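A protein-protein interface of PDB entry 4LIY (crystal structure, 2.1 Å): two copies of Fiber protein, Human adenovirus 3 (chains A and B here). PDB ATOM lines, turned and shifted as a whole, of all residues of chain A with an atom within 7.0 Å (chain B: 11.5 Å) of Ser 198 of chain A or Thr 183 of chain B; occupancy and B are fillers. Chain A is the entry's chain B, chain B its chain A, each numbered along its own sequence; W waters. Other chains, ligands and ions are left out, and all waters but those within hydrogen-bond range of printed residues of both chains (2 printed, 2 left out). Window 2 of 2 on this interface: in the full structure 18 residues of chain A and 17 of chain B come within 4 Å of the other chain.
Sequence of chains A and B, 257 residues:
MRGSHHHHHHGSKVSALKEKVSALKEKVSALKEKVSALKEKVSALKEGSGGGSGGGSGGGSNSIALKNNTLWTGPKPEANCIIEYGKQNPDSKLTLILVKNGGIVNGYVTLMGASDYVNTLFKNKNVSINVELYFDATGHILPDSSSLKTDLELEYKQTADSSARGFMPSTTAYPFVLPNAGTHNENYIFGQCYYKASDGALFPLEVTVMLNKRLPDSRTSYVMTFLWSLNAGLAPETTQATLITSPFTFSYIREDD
ND2 of Asn 185 of chain B sits at hydrogen-bond distance from O of Lys 196 of chain A (2.9 Å).
NZ of Lys 196 of chain A lies within hydrogen-bond range of O of Gly 200 of chain A (3.0 Å).
The side-chain carboxylate (OE2) of Glu 237 of chain A is in hydrogen-bond range of the backbone NH (N) of Ser 198 of chain A (2.8 Å).
Among the printed residues, merely in contact across the chains: Ala 197 of chain A with Thr 183 of chain B (3.4 Å), Lys 196 of chain A with Phe 190 of chain B (3.5 Å), Ile 244 of chain A with Asn 185 of chain B (3.6 Å), Ser 198 of chain A with Thr 183 of chain B (3.7 Å) and Ile 244 of chain A with Glu 186 of chain B (3.7 Å).
Ser 198 of chain A touches one residue of chain B.
Lys 196 of chain A touches just these residues of chain B: Asn 185 (2.9 Å) and Phe 190 (3.5 Å).
No residue of chain B comes within 4 Å of Asp 199 of chain A.
Gly 200 of chain A touches none of the printed residues of chain B.
No residue of chain B comes within 4 Å of Ala 201 of chain A.
Printed residues of chain A within 4 Å of Phe 190 of chain B: Lys 196.
Of the printed residues of chain B, Ile 244 of chain A touches Asn 185 and Glu 186.
Of the printed residues of chain A, Asn 185 of chain B touches Lys 196 (2.9 Å) and Ile 244 (3.6 Å).
The nearest residue of chain B that does not touch Ser 198 of chain A is Gly 182 of chain B (6.0 Å).
The nearest printed residue of chain A that does not touch Asn 185 of chain B is Tyr 195 of chain A (4.4 Å).
Of the 24 printed residues of chain B, 4 touch a printed residue of chain A.
Hydrophobic or aromatic side chains of chain B that line the printed part of chain A: Phe 190.
Hydrophobic or aromatic side chains of chain A within 4 Å of the printed part of chain B: Ile 244.
Among the printed residues, no Asp or Glu carboxylate lies within 4 Å of a Lys or Arg side-chain nitrogen of the other chain.
No position is printed for both chains.
Of the 6 pairs that touch across the chains among the printed residues, none has its exchanged pair printed and touching as well.
Water W2 lies within hydrogen-bond range of O of Thr 242 of chain A (2.5 Å) and ND2 of Asn 185 of chain B (3.1 Å).
Water W1 lies within hydrogen-bond range of the backbone carbonyl oxygen of Ile 244 of chain A, the backbone NH of Lys 196 of chain A and the side-chain amide oxygen of Asn 185 of chain B.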
ATOM      1  N   TYR A 195      14.405 -17.198 -14.202  1.00  0.00           N
ATOM      2  CA  TYR A 195      14.372 -17.303 -15.651  1.00  0.00           C
ATOM      3  C   TYR A 195      14.085 -18.752 -16.050  1.00  0.00           C
ATOM      4  O   TYR A 195      14.811 -19.665 -15.647  1.00  0.00           O
ATOM      5  CB  TYR A 195      15.702 -16.852 -16.244  1.00  0.00           C
ATOM      6  CG  TYR A 195      15.814 -17.098 -17.736  1.00  0.00           C
ATOM      7  CD1 TYR A 195      15.144 -16.286 -18.642  1.00  0.00           C
ATOM      8  CD2 TYR A 195      16.566 -18.162 -18.238  1.00  0.00           C
ATOM      9  CE1 TYR A 195      15.228 -16.508 -20.003  1.00  0.00           C
ATOM     10  CE2 TYR A 195      16.666 -18.393 -19.603  1.00  0.00           C
ATOM     11  CZ  TYR A 195      15.992 -17.567 -20.481  1.00  0.00           C
ATOM     12  OH  TYR A 195      16.079 -17.789 -21.844  1.00  0.00           O
ATOM     13  N   LYS A 196      13.028 -18.956 -16.829  1.00  0.00           N
ATOM     14  CA  LYS A 196      12.714 -20.290 -17.338  1.00  0.00           C
ATOM     15  C   LYS A 196      13.316 -20.427 -18.725  1.00  0.00           C
ATOM     16  O   LYS A 196      12.952 -19.712 -19.657  1.00  0.00           O
ATOM     17  CB  LYS A 196      11.212 -20.537 -17.361  1.00  0.00           C
ATOM     18  CG  LYS A 196      10.814 -21.869 -17.999  1.00  0.00           C
ATOM     19  CD  LYS A 196       9.303 -22.100 -17.987  1.00  0.00           C
ATOM     20  CE  LYS A 196       8.813 -22.680 -16.653  1.00  0.00           C
ATOM     21  NZ  LYS A 196       9.478 -23.952 -16.239  1.00  0.00           N
ATOM     22  N   ALA A 197      14.269 -21.336 -18.849  1.00  0.00           N
ATOM     23  CA  ALA A 197      14.989 -21.512 -20.089  1.00  0.00           C
ATOM     24  C   ALA A 197      14.096 -22.269 -21.081  1.00  0.00           C
ATOM     25  O   ALA A 197      13.064 -22.794 -20.686  1.00  0.00           O
ATOM     26  CB  ALA A 197      16.270 -22.294 -19.826  1.00  0.00           C
ATOM     27  N   SER A 198      14.498 -22.320 -22.352  1.00  0.00           N
ATOM     28  CA  SER A 198      13.705 -22.960 -23.414  1.00  0.00           C
ATOM     29  C   SER A 198      13.403 -24.447 -23.180  1.00  0.00           C
ATOM     30  O   SER A 198      12.361 -24.935 -23.610  1.00  0.00           O
ATOM     31  CB  SER A 198      14.410 -22.793 -24.765  1.00  0.00           C
ATOM     32  OG  SER A 198      14.467 -21.433 -25.142  1.00  0.00           O
ATOM     33  N   ASP A 199      14.310 -25.154 -22.504  1.00  0.00           N
ATOM     34  CA  ASP A 199      14.136 -26.571 -22.185  1.00  0.00           C
ATOM     35  C   ASP A 199      13.349 -26.756 -20.891  1.00  0.00           C
ATOM     36  O   ASP A 199      13.264 -27.865 -20.353  1.00  0.00           O
ATOM     37  CB  ASP A 199      15.499 -27.300 -22.102  1.00  0.00           C
ATOM     38  CG  ASP A 199      16.395 -26.790 -20.968  1.00  0.00           C
ATOM     39  OD1 ASP A 199      16.086 -25.737 -20.343  1.00  0.00           O
ATOM     40  OD2 ASP A 199      17.433 -27.449 -20.715  1.00  0.00           O
ATOM     41  N   GLY A 200      12.784 -25.662 -20.380  1.00  0.00           N
ATOM     42  CA  GLY A 200      11.913 -25.729 -19.218  1.00  0.00           C
ATOM     43  C   GLY A 200      12.600 -25.652 -17.860  1.00  0.00           C
ATOM     44  O   GLY A 200      11.924 -25.598 -16.835  1.00  0.00           O
ATOM     45  N   ALA A 201      13.931 -25.644 -17.840  1.00  0.00           N
ATOM     46  CA  ALA A 201      14.673 -25.545 -16.580  1.00  0.00           C
ATOM     47  C   ALA A 201      14.505 -24.146 -15.940  1.00  0.00           C
ATOM     48  O   ALA A 201      14.608 -23.123 -16.608  1.00  0.00           O
ATOM     49  CB  ALA A 201      16.154 -25.855 -16.808  1.00  0.00           C
ATOM     50  N   PRO A 236      21.496 -21.539 -19.198  1.00  0.00           N
ATOM     51  CA  PRO A 236      20.109 -21.855 -19.513  1.00  0.00           C
ATOM     52  C   PRO A 236      19.939 -22.175 -21.000  1.00  0.00           C
ATOM     53  O   PRO A 236      19.108 -23.014 -21.310  1.00  0.00           O
ATOM     54  CB  PRO A 236      19.380 -20.572 -19.111  1.00  0.00           C
ATOM     55  CG  PRO A 236      20.290 -19.948 -18.081  1.00  0.00           C
ATOM     56  CD  PRO A 236      21.639 -20.230 -18.542  1.00  0.00           C
ATOM     57  N   GLU A 237      20.737 -21.556 -21.873  1.00  0.00           N
ATOM     58  CA  GLU A 237      20.483 -21.595 -23.318  1.00  0.00           C
ATOM     59  C   GLU A 237      21.704 -21.941 -24.158  1.00  0.00           C
ATOM     60  O   GLU A 237      22.830 -21.605 -23.804  1.00  0.00           O
ATOM     61  CB  GLU A 237      19.950 -20.242 -23.800  1.00  0.00           C
ATOM     62  CG  GLU A 237      18.712 -19.722 -23.040  1.00  0.00           C
ATOM     63  CD  GLU A 237      17.480 -20.558 -23.281  1.00  0.00           C
ATOM     64  OE1 GLU A 237      17.561 -21.487 -24.100  1.00  0.00           O
ATOM     65  OE2 GLU A 237      16.426 -20.279 -22.663  1.00  0.00           O
ATOM     66  N   THR A 239      21.068 -21.299 -27.545  1.00  0.00           N
ATOM     67  CA  THR A 239      20.717 -20.387 -28.629  1.00  0.00           C
ATOM     68  C   THR A 239      19.972 -19.151 -28.140  1.00  0.00           C
ATOM     69  O   THR A 239      19.636 -19.024 -26.964  1.00  0.00           O
ATOM     70  CB  THR A 239      19.776 -21.059 -29.629  1.00  0.00           C
ATOM     71  OG1 THR A 239      18.472 -21.179 -29.047  1.00  0.00           O
ATOM     72  CG2 THR A 239      20.281 -22.427 -30.013  1.00  0.00           C
ATOM     73  N   GLN A 240      19.684 -18.268 -29.086  1.00  0.00           N
ATOM     74  CA  GLN A 240      18.903 -17.076 -28.837  1.00  0.00           C
ATOM     75  C   GLN A 240      17.490 -17.435 -28.376  1.00  0.00           C
ATOM     76  O   GLN A 240      16.850 -18.331 -28.915  1.00  0.00           O
ATOM     77  CB  GLN A 240      18.836 -16.241 -30.105  1.00  0.00           C
ATOM     78  CG  GLN A 240      17.911 -15.056 -29.992  1.00  0.00           C
ATOM     79  CD  GLN A 240      18.239 -13.948 -30.970  1.00  0.00           C
ATOM     80  OE1 GLN A 240      19.320 -13.912 -31.550  1.00  0.00           O
ATOM     81  NE2 GLN A 240      17.298 -13.037 -31.163  1.00  0.00           N
ATOM     82  N   ALA A 241      17.017 -16.720 -27.362  1.00  0.00           N
ATOM     83  CA  ALA A 241      15.697 -16.946 -26.801  1.00  0.00           C
ATOM     84  C   ALA A 241      15.318 -15.648 -26.109  1.00  0.00           C
ATOM     85  O   ALA A 241      16.192 -14.915 -25.654  1.00  0.00           O
ATOM     86  CB  ALA A 241      15.729 -18.092 -25.805  1.00  0.00           C
ATOM     87  N   THR A 242      14.030 -15.346 -26.039  1.00  0.00           N
ATOM     88  CA  THR A 242      13.610 -14.078 -25.463  1.00  0.00           C
ATOM     89  C   THR A 242      13.946 -14.019 -23.976  1.00  0.00           C
ATOM     90  O   THR A 242      13.458 -14.811 -23.172  1.00  0.00           O
ATOM     91  CB  THR A 242      12.121 -13.838 -25.698  1.00  0.00           C
ATOM     92  OG1 THR A 242      11.867 -13.849 -27.110  1.00  0.00           O
ATOM     93  CG2 THR A 242      11.707 -12.498 -25.143  1.00  0.00           C
ATOM     94  N   ILE A 244      13.435 -13.020 -20.452  1.00  0.00           N
ATOM     95  CA  ILE A 244      12.339 -12.504 -19.641  1.00  0.00           C
ATOM     96  C   ILE A 244      12.639 -12.817 -18.197  1.00  0.00           C
ATOM     97  O   ILE A 244      12.732 -13.992 -17.839  1.00  0.00           O
ATOM     98  CB  ILE A 244      11.006 -13.161 -19.999  1.00  0.00           C
ATOM     99  CG1 ILE A 244      10.624 -12.824 -21.437  1.00  0.00           C
ATOM    100  CG2 ILE A 244       9.907 -12.685 -19.031  1.00  0.00           C
ATOM    101  CD1 ILE A 244       9.406 -13.598 -21.977  1.00  0.00           C
ATOM    102  N   TYR B 174      -0.823 -10.236 -19.586  1.00  0.00           N
ATOM    103  CA  TYR B 174      -0.744 -11.696 -19.580  1.00  0.00           C
ATOM    104  C   TYR B 174      -1.732 -12.204 -20.617  1.00  0.00           C
ATOM    105  O   TYR B 174      -2.889 -12.528 -20.300  1.00  0.00           O
ATOM    106  CB  TYR B 174      -1.056 -12.250 -18.195  1.00  0.00           C
ATOM    107  CG  TYR B 174      -0.412 -11.424 -17.094  1.00  0.00           C
ATOM    108  CD1 TYR B 174       0.965 -11.478 -16.865  1.00  0.00           C
ATOM    109  CD2 TYR B 174      -1.170 -10.576 -16.305  1.00  0.00           C
ATOM    110  CE1 TYR B 174       1.560 -10.714 -15.861  1.00  0.00           C
ATOM    111  CE2 TYR B 174      -0.585  -9.827 -15.290  1.00  0.00           C
ATOM    112  CZ  TYR B 174       0.781  -9.899 -15.085  1.00  0.00           C
ATOM    113  OH  TYR B 174       1.373  -9.157 -14.102  1.00  0.00           O
ATOM    114  N   PRO B 175      -1.294 -12.214 -21.874  1.00  0.00           N
ATOM    115  CA  PRO B 175      -2.200 -12.514 -22.983  1.00  0.00           C
ATOM    116  C   PRO B 175      -2.562 -13.998 -23.074  1.00  0.00           C
ATOM    117  O   PRO B 175      -1.852 -14.851 -22.531  1.00  0.00           O
ATOM    118  CB  PRO B 175      -1.396 -12.094 -24.216  1.00  0.00           C
ATOM    119  CG  PRO B 175       0.046 -12.279 -23.799  1.00  0.00           C
ATOM    120  CD  PRO B 175       0.079 -11.908 -22.332  1.00  0.00           C
ATOM    121  N   VAL B 177      -2.754 -17.023 -25.699  1.00  0.00           N
ATOM    122  CA  VAL B 177      -2.000 -17.298 -26.907  1.00  0.00           C
ATOM    123  C   VAL B 177      -2.411 -18.635 -27.514  1.00  0.00           C
ATOM    124  O   VAL B 177      -3.147 -19.413 -26.908  1.00  0.00           O
ATOM    125  CB  VAL B 177      -0.474 -17.292 -26.633  1.00  0.00           C
ATOM    126  CG1 VAL B 177      -0.047 -15.943 -26.007  1.00  0.00           C
ATOM    127  CG2 VAL B 177      -0.072 -18.437 -25.706  1.00  0.00           C
ATOM    128  N   LEU B 178      -1.927 -18.887 -28.718  1.00  0.00           N
ATOM    129  CA  LEU B 178      -2.177 -20.151 -29.381  1.00  0.00           C
ATOM    130  C   LEU B 178      -1.612 -21.302 -28.536  1.00  0.00           C
ATOM    131  O   LEU B 178      -0.579 -21.150 -27.888  1.00  0.00           O
ATOM    132  CB  LEU B 178      -1.543 -20.129 -30.752  1.00  0.00           C
ATOM    133  CG  LEU B 178      -2.258 -19.254 -31.781  1.00  0.00           C
ATOM    134  CD1 LEU B 178      -1.387 -19.130 -32.991  1.00  0.00           C
ATOM    135  CD2 LEU B 178      -3.602 -19.835 -32.195  1.00  0.00           C
ATOM    136  N   PRO B 179      -2.305 -22.446 -28.519  1.00  0.00           N
ATOM    137  CA  PRO B 179      -1.917 -23.588 -27.681  1.00  0.00           C
ATOM    138  C   PRO B 179      -0.700 -24.296 -28.279  1.00  0.00           C
ATOM    139  O   PRO B 179      -0.763 -25.476 -28.662  1.00  0.00           O
ATOM    140  CB  PRO B 179      -3.172 -24.475 -27.716  1.00  0.00           C
ATOM    141  CG  PRO B 179      -3.753 -24.205 -29.104  1.00  0.00           C
ATOM    142  CD  PRO B 179      -3.456 -22.756 -29.385  1.00  0.00           C
ATOM    143  N   ASN B 180       0.402 -23.563 -28.391  1.00  0.00           N
ATOM    144  CA  ASN B 180       1.649 -24.125 -28.894  1.00  0.00           C
ATOM    145  C   ASN B 180       2.592 -24.365 -27.738  1.00  0.00           C
ATOM    146  O   ASN B 180       2.683 -23.529 -26.829  1.00  0.00           O
ATOM    147  CB  ASN B 180       2.330 -23.164 -29.871  1.00  0.00           C
ATOM    148  CG  ASN B 180       1.646 -23.105 -31.205  1.00  0.00           C
ATOM    149  OD1 ASN B 180       1.083 -24.099 -31.666  1.00  0.00           O
ATOM    150  ND2 ASN B 180       1.698 -21.945 -31.851  1.00  0.00           N
ATOM    151  N   ALA B 181       3.349 -25.459 -27.802  1.00  0.00           N
ATOM    152  CA  ALA B 181       4.380 -25.735 -26.791  1.00  0.00           C
ATOM    153  C   ALA B 181       5.310 -24.530 -26.700  1.00  0.00           C
ATOM    154  O   ALA B 181       5.496 -23.815 -27.671  1.00  0.00           O
ATOM    155  CB  ALA B 181       5.178 -26.955 -27.175  1.00  0.00           C
ATOM    156  N   GLY B 182       5.906 -24.285 -25.552  1.00  0.00           N
ATOM    157  CA  GLY B 182       6.753 -23.110 -25.435  1.00  0.00           C
ATOM    158  C   GLY B 182       6.792 -22.676 -24.002  1.00  0.00           C
ATOM    159  O   GLY B 182       6.031 -23.185 -23.186  1.00  0.00           O
ATOM    160  N   THR B 183       7.667 -21.733 -23.695  1.00  0.00           N
ATOM    161  CA  THR B 183       7.894 -21.337 -22.310  1.00  0.00           C
ATOM    162  C   THR B 183       6.908 -20.246 -21.858  1.00  0.00           C
ATOM    163  O   THR B 183       6.488 -20.232 -20.698  1.00  0.00           O
ATOM    164  CB  THR B 183       9.346 -20.867 -22.130  1.00  0.00           C
ATOM    165  OG1 THR B 183       9.610 -19.790 -23.039  1.00  0.00           O
ATOM    166  CG2 THR B 183      10.303 -22.013 -22.425  1.00  0.00           C
ATOM    167  N   HIS B 184       6.558 -19.346 -22.782  1.00  0.00           N
ATOM    168  CA  HIS B 184       5.543 -18.300 -22.570  1.00  0.00           C
ATOM    169  C   HIS B 184       5.764 -17.569 -21.286  1.00  0.00           C
ATOM    170  O   HIS B 184       4.820 -17.299 -20.549  1.00  0.00           O
ATOM    171  CB  HIS B 184       4.144 -18.912 -22.578  1.00  0.00           C
ATOM    172  CG  HIS B 184       3.848 -19.663 -23.836  1.00  0.00           C
ATOM    173  ND1 HIS B 184       3.618 -19.031 -25.037  1.00  0.00           N
ATOM    174  CD2 HIS B 184       3.796 -20.990 -24.091  1.00  0.00           C
ATOM    175  CE1 HIS B 184       3.417 -19.939 -25.979  1.00  0.00           C
ATOM    176  NE2 HIS B 184       3.519 -21.135 -25.429  1.00  0.00           N
ATOM    177  N   ASN B 185       7.027 -17.271 -21.024  1.00  0.00           N
ATOM    178  CA  ASN B 185       7.437 -16.758 -19.729  1.00  0.00           C
ATOM    179  C   ASN B 185       6.609 -15.590 -19.242  1.00  0.00           C
ATOM    180  O   ASN B 185       6.386 -15.462 -18.041  1.00  0.00           O
ATOM    181  CB  ASN B 185       8.920 -16.378 -19.762  1.00  0.00           C
ATOM    182  CG  ASN B 185       9.815 -17.554 -19.474  1.00  0.00           C
ATOM    183  OD1 ASN B 185       9.429 -18.426 -18.709  1.00  0.00           O
ATOM    184  ND2 ASN B 185      11.012 -17.588 -20.073  1.00  0.00           N
ATOM    185  N   GLU B 186       6.114 -14.764 -20.159  1.00  0.00           N
ATOM    186  CA  GLU B 186       5.440 -13.531 -19.752  1.00  0.00           C
ATOM    187  C   GLU B 186       4.184 -13.833 -18.925  1.00  0.00           C
ATOM    188  O   GLU B 186       3.728 -12.991 -18.188  1.00  0.00           O
ATOM    189  CB  GLU B 186       5.122 -12.610 -20.948  1.00  0.00           C
ATOM    190  CG  GLU B 186       4.511 -13.304 -22.130  1.00  0.00           C
ATOM    191  CD  GLU B 186       5.533 -13.613 -23.210  1.00  0.00           C
ATOM    192  OE1 GLU B 186       6.063 -14.750 -23.215  1.00  0.00           O
ATOM    193  OE2 GLU B 186       5.804 -12.716 -24.044  1.00  0.00           O
ATOM    194  N   ASN B 187       3.658 -15.049 -19.025  1.00  0.00           N
ATOM    195  CA  ASN B 187       2.441 -15.421 -18.315  1.00  0.00           C
ATOM    196  C   ASN B 187       2.696 -16.070 -16.955  1.00  0.00           C
ATOM    197  O   ASN B 187       1.745 -16.505 -16.285  1.00  0.00           O
ATOM    198  CB  ASN B 187       1.611 -16.388 -19.172  1.00  0.00           C
ATOM    199  CG  ASN B 187       1.079 -15.731 -20.414  1.00  0.00           C
ATOM    200  OD1 ASN B 187       1.756 -15.717 -21.441  1.00  0.00           O
ATOM    201  ND2 ASN B 187      -0.127 -15.163 -20.334  1.00  0.00           N
ATOM    202  N   TYR B 188       3.959 -16.153 -16.545  1.00  0.00           N
ATOM    203  CA  TYR B 188       4.292 -16.886 -15.317  1.00  0.00           C
ATOM    204  C   TYR B 188       4.949 -16.020 -14.233  1.00  0.00           C
ATOM    205  O   TYR B 188       5.823 -15.206 -14.510  1.00  0.00           O
ATOM    206  CB  TYR B 188       5.209 -18.063 -15.640  1.00  0.00           C
ATOM    207  CG  TYR B 188       4.517 -19.199 -16.416  1.00  0.00           C
ATOM    208  CD1 TYR B 188       3.706 -20.117 -15.763  1.00  0.00           C
ATOM    209  CD2 TYR B 188       4.660 -19.326 -17.790  1.00  0.00           C
ATOM    210  CE1 TYR B 188       3.060 -21.150 -16.457  1.00  0.00           C
ATOM    211  CE2 TYR B 188       4.012 -20.377 -18.506  1.00  0.00           C
ATOM    212  CZ  TYR B 188       3.222 -21.266 -17.826  1.00  0.00           C
ATOM    213  OH  TYR B 188       2.595 -22.269 -18.504  1.00  0.00           O
ATOM    214  N   ILE B 189       4.524 -16.243 -12.996  1.00  0.00           N
ATOM    215  CA  ILE B 189       5.193 -15.734 -11.823  1.00  0.00           C
ATOM    216  C   ILE B 189       5.786 -16.917 -11.062  1.00  0.00           C
ATOM    217  O   ILE B 189       5.080 -17.883 -10.779  1.00  0.00           O
ATOM    218  CB  ILE B 189       4.175 -15.024 -10.907  1.00  0.00           C
ATOM    219  CG1 ILE B 189       3.670 -13.752 -11.573  1.00  0.00           C
ATOM    220  CG2 ILE B 189       4.794 -14.705  -9.563  1.00  0.00           C
ATOM    221  CD1 ILE B 189       2.479 -13.142 -10.865  1.00  0.00           C
ATOM    222  N   PHE B 190       7.068 -16.857 -10.721  1.00  0.00           N
ATOM    223  CA  PHE B 190       7.691 -17.930  -9.939  1.00  0.00           C
ATOM    224  C   PHE B 190       8.092 -17.402  -8.564  1.00  0.00           C
ATOM    225  O   PHE B 190       8.493 -16.242  -8.417  1.00  0.00           O
ATOM    226  CB  PHE B 190       8.915 -18.481 -10.666  1.00  0.00           C
ATOM    227  CG  PHE B 190       8.619 -19.003 -12.053  1.00  0.00           C
ATOM    228  CD1 PHE B 190       8.062 -20.256 -12.233  1.00  0.00           C
ATOM    229  CD2 PHE B 190       8.916 -18.252 -13.176  1.00  0.00           C
ATOM    230  CE1 PHE B 190       7.786 -20.743 -13.506  1.00  0.00           C
ATOM    231  CE2 PHE B 190       8.642 -18.745 -14.449  1.00  0.00           C
ATOM    232  CZ  PHE B 190       8.073 -19.987 -14.610  1.00  0.00           C
ATOM    233  N   THR B 208       4.609 -21.947  -8.851  1.00  0.00           N
ATOM    234  CA  THR B 208       4.413 -21.422 -10.187  1.00  0.00           C
ATOM    235  C   THR B 208       2.975 -20.917 -10.290  1.00  0.00           C
ATOM    236  O   THR B 208       2.034 -21.650  -9.978  1.00  0.00           O
ATOM    237  CB  THR B 208       4.678 -22.494 -11.234  1.00  0.00           C
ATOM    238  OG1 THR B 208       6.022 -22.959 -11.076  1.00  0.00           O
ATOM    239  CG2 THR B 208       4.509 -21.936 -12.641  1.00  0.00           C
ATOM    240  N   VAL B 209       2.822 -19.644 -10.651  1.00  0.00           N
ATOM    241  CA  VAL B 209       1.515 -19.057 -10.936  1.00  0.00           C
ATOM    242  C   VAL B 209       1.435 -18.746 -12.423  1.00  0.00           C
ATOM    243  O   VAL B 209       2.312 -18.056 -12.958  1.00  0.00           O
ATOM    244  CB  VAL B 209       1.291 -17.763 -10.174  1.00  0.00           C
ATOM    245  CG1 VAL B 209      -0.117 -17.261 -10.421  1.00  0.00           C
ATOM    246  CG2 VAL B 209       1.523 -17.978  -8.675  1.00  0.00           C
ATOM    247  N   MET B 210       0.420 -19.299 -13.093  1.00  0.00           N
ATOM    248  CA  MET B 210       0.154 -18.983 -14.483  1.00  0.00           C
ATOM    249  C   MET B 210      -1.057 -18.070 -14.584  1.00  0.00           C
ATOM    250  O   MET B 210      -2.098 -18.319 -13.969  1.00  0.00           O
ATOM    251  CB  MET B 210      -0.142 -20.252 -15.307  1.00  0.00           C
ATOM    252  CG  MET B 210      -0.168 -19.962 -16.797  1.00  0.00           C
ATOM    253  SD  MET B 210      -0.664 -21.381 -17.819  1.00  0.00           S
ATOM    254  CE  MET B 210      -2.423 -21.430 -17.551  1.00  0.00           C
ATOM    255  N   LEU B 211      -0.934 -17.037 -15.401  1.00  0.00           N
ATOM    256  CA  LEU B 211      -2.016 -16.097 -15.601  1.00  0.00           C
ATOM    257  C   LEU B 211      -2.456 -16.136 -17.053  1.00  0.00           C
ATOM    258  O   LEU B 211      -1.647 -15.958 -17.968  1.00  0.00           O
ATOM    259  CB  LEU B 211      -1.572 -14.693 -15.219  1.00  0.00           C
ATOM    260  CG  LEU B 211      -1.136 -14.568 -13.760  1.00  0.00           C
ATOM    261  CD1 LEU B 211      -0.643 -13.188 -13.477  1.00  0.00           C
ATOM    262  CD2 LEU B 211      -2.278 -14.924 -12.815  1.00  0.00           C
ATOM    263  N   ASN B 212      -3.750 -16.342 -17.241  1.00  0.00           N
ATOM    264  CA  ASN B 212      -4.335 -16.421 -18.561  1.00  0.00           C
ATOM    265  C   ASN B 212      -3.570 -17.456 -19.423  1.00  0.00           C
ATOM    266  O   ASN B 212      -3.509 -18.619 -19.040  1.00  0.00           O
ATOM    267  CB  ASN B 212      -4.405 -15.020 -19.158  1.00  0.00           C
ATOM    268  CG  ASN B 212      -5.289 -14.081 -18.336  1.00  0.00           C
ATOM    269  OD1 ASN B 212      -6.267 -14.516 -17.705  1.00  0.00           O
ATOM    270  ND2 ASN B 212      -4.944 -12.787 -18.327  1.00  0.00           N
ATOM    271  N   LYS B 213      -2.993 -17.029 -20.549  1.00  0.00           N
ATOM    272  CA  LYS B 213      -2.178 -17.870 -21.436  1.00  0.00           C
ATOM    273  C   LYS B 213      -3.016 -18.887 -22.236  1.00  0.00           C
ATOM    274  O   LYS B 213      -3.042 -18.848 -23.457  1.00  0.00           O
ATOM    275  CB  LYS B 213      -1.049 -18.618 -20.707  1.00  0.00           C
ATOM    276  CG  LYS B 213       0.053 -19.099 -21.678  1.00  0.00           C
ATOM    277  CD  LYS B 213       0.842 -20.295 -21.163  1.00  0.00           C
ATOM    278  CE  LYS B 213       0.074 -21.607 -21.339  1.00  0.00           C
ATOM    279  NZ  LYS B 213       0.858 -22.782 -20.850  1.00  0.00           N
ATOM    280  N   ARG B 214      -3.699 -19.785 -21.547  1.00  0.00           N
ATOM    281  CA  ARG B 214      -4.378 -20.888 -22.231  1.00  0.00           C
ATOM    282  C   ARG B 214      -5.851 -20.942 -21.844  1.00  0.00           C
ATOM    283  O   ARG B 214      -6.181 -21.247 -20.696  1.00  0.00           O
ATOM    284  CB  ARG B 214      -3.693 -22.219 -21.901  1.00  0.00           C
ATOM    285  CG  ARG B 214      -4.407 -23.469 -22.484  1.00  0.00           C
ATOM    286  CD  ARG B 214      -4.066 -23.689 -23.954  1.00  0.00           C
ATOM    287  NE  ARG B 214      -4.805 -24.810 -24.563  1.00  0.00           N
ATOM    288  CZ  ARG B 214      -5.950 -24.686 -25.242  1.00  0.00           C
ATOM    289  NH1 ARG B 214      -6.515 -23.491 -25.402  1.00  0.00           N
ATOM    290  NH2 ARG B 214      -6.538 -25.759 -25.765  1.00  0.00           N
ATOM    291  N   THR B 225      -3.757 -20.182 -12.351  1.00  0.00           N
ATOM    292  CA  THR B 225      -3.437 -21.513 -11.837  1.00  0.00           C
ATOM    293  C   THR B 225      -2.242 -21.430 -10.911  1.00  0.00           C
ATOM    294  O   THR B 225      -1.372 -20.552 -11.076  1.00  0.00           O
ATOM    295  CB  THR B 225      -3.135 -22.534 -12.966  1.00  0.00           C
ATOM    296  OG1 THR B 225      -1.834 -22.280 -13.509  1.00  0.00           O
ATOM    297  CG2 THR B 225      -4.188 -22.472 -14.071  1.00  0.00           C
HETATM  298  O   HOH W   1      11.338 -16.470 -17.043  1.00  0.00           O
HETATM  299  O   HOH W   2      11.856 -16.717 -22.906  1.00  0.00           O
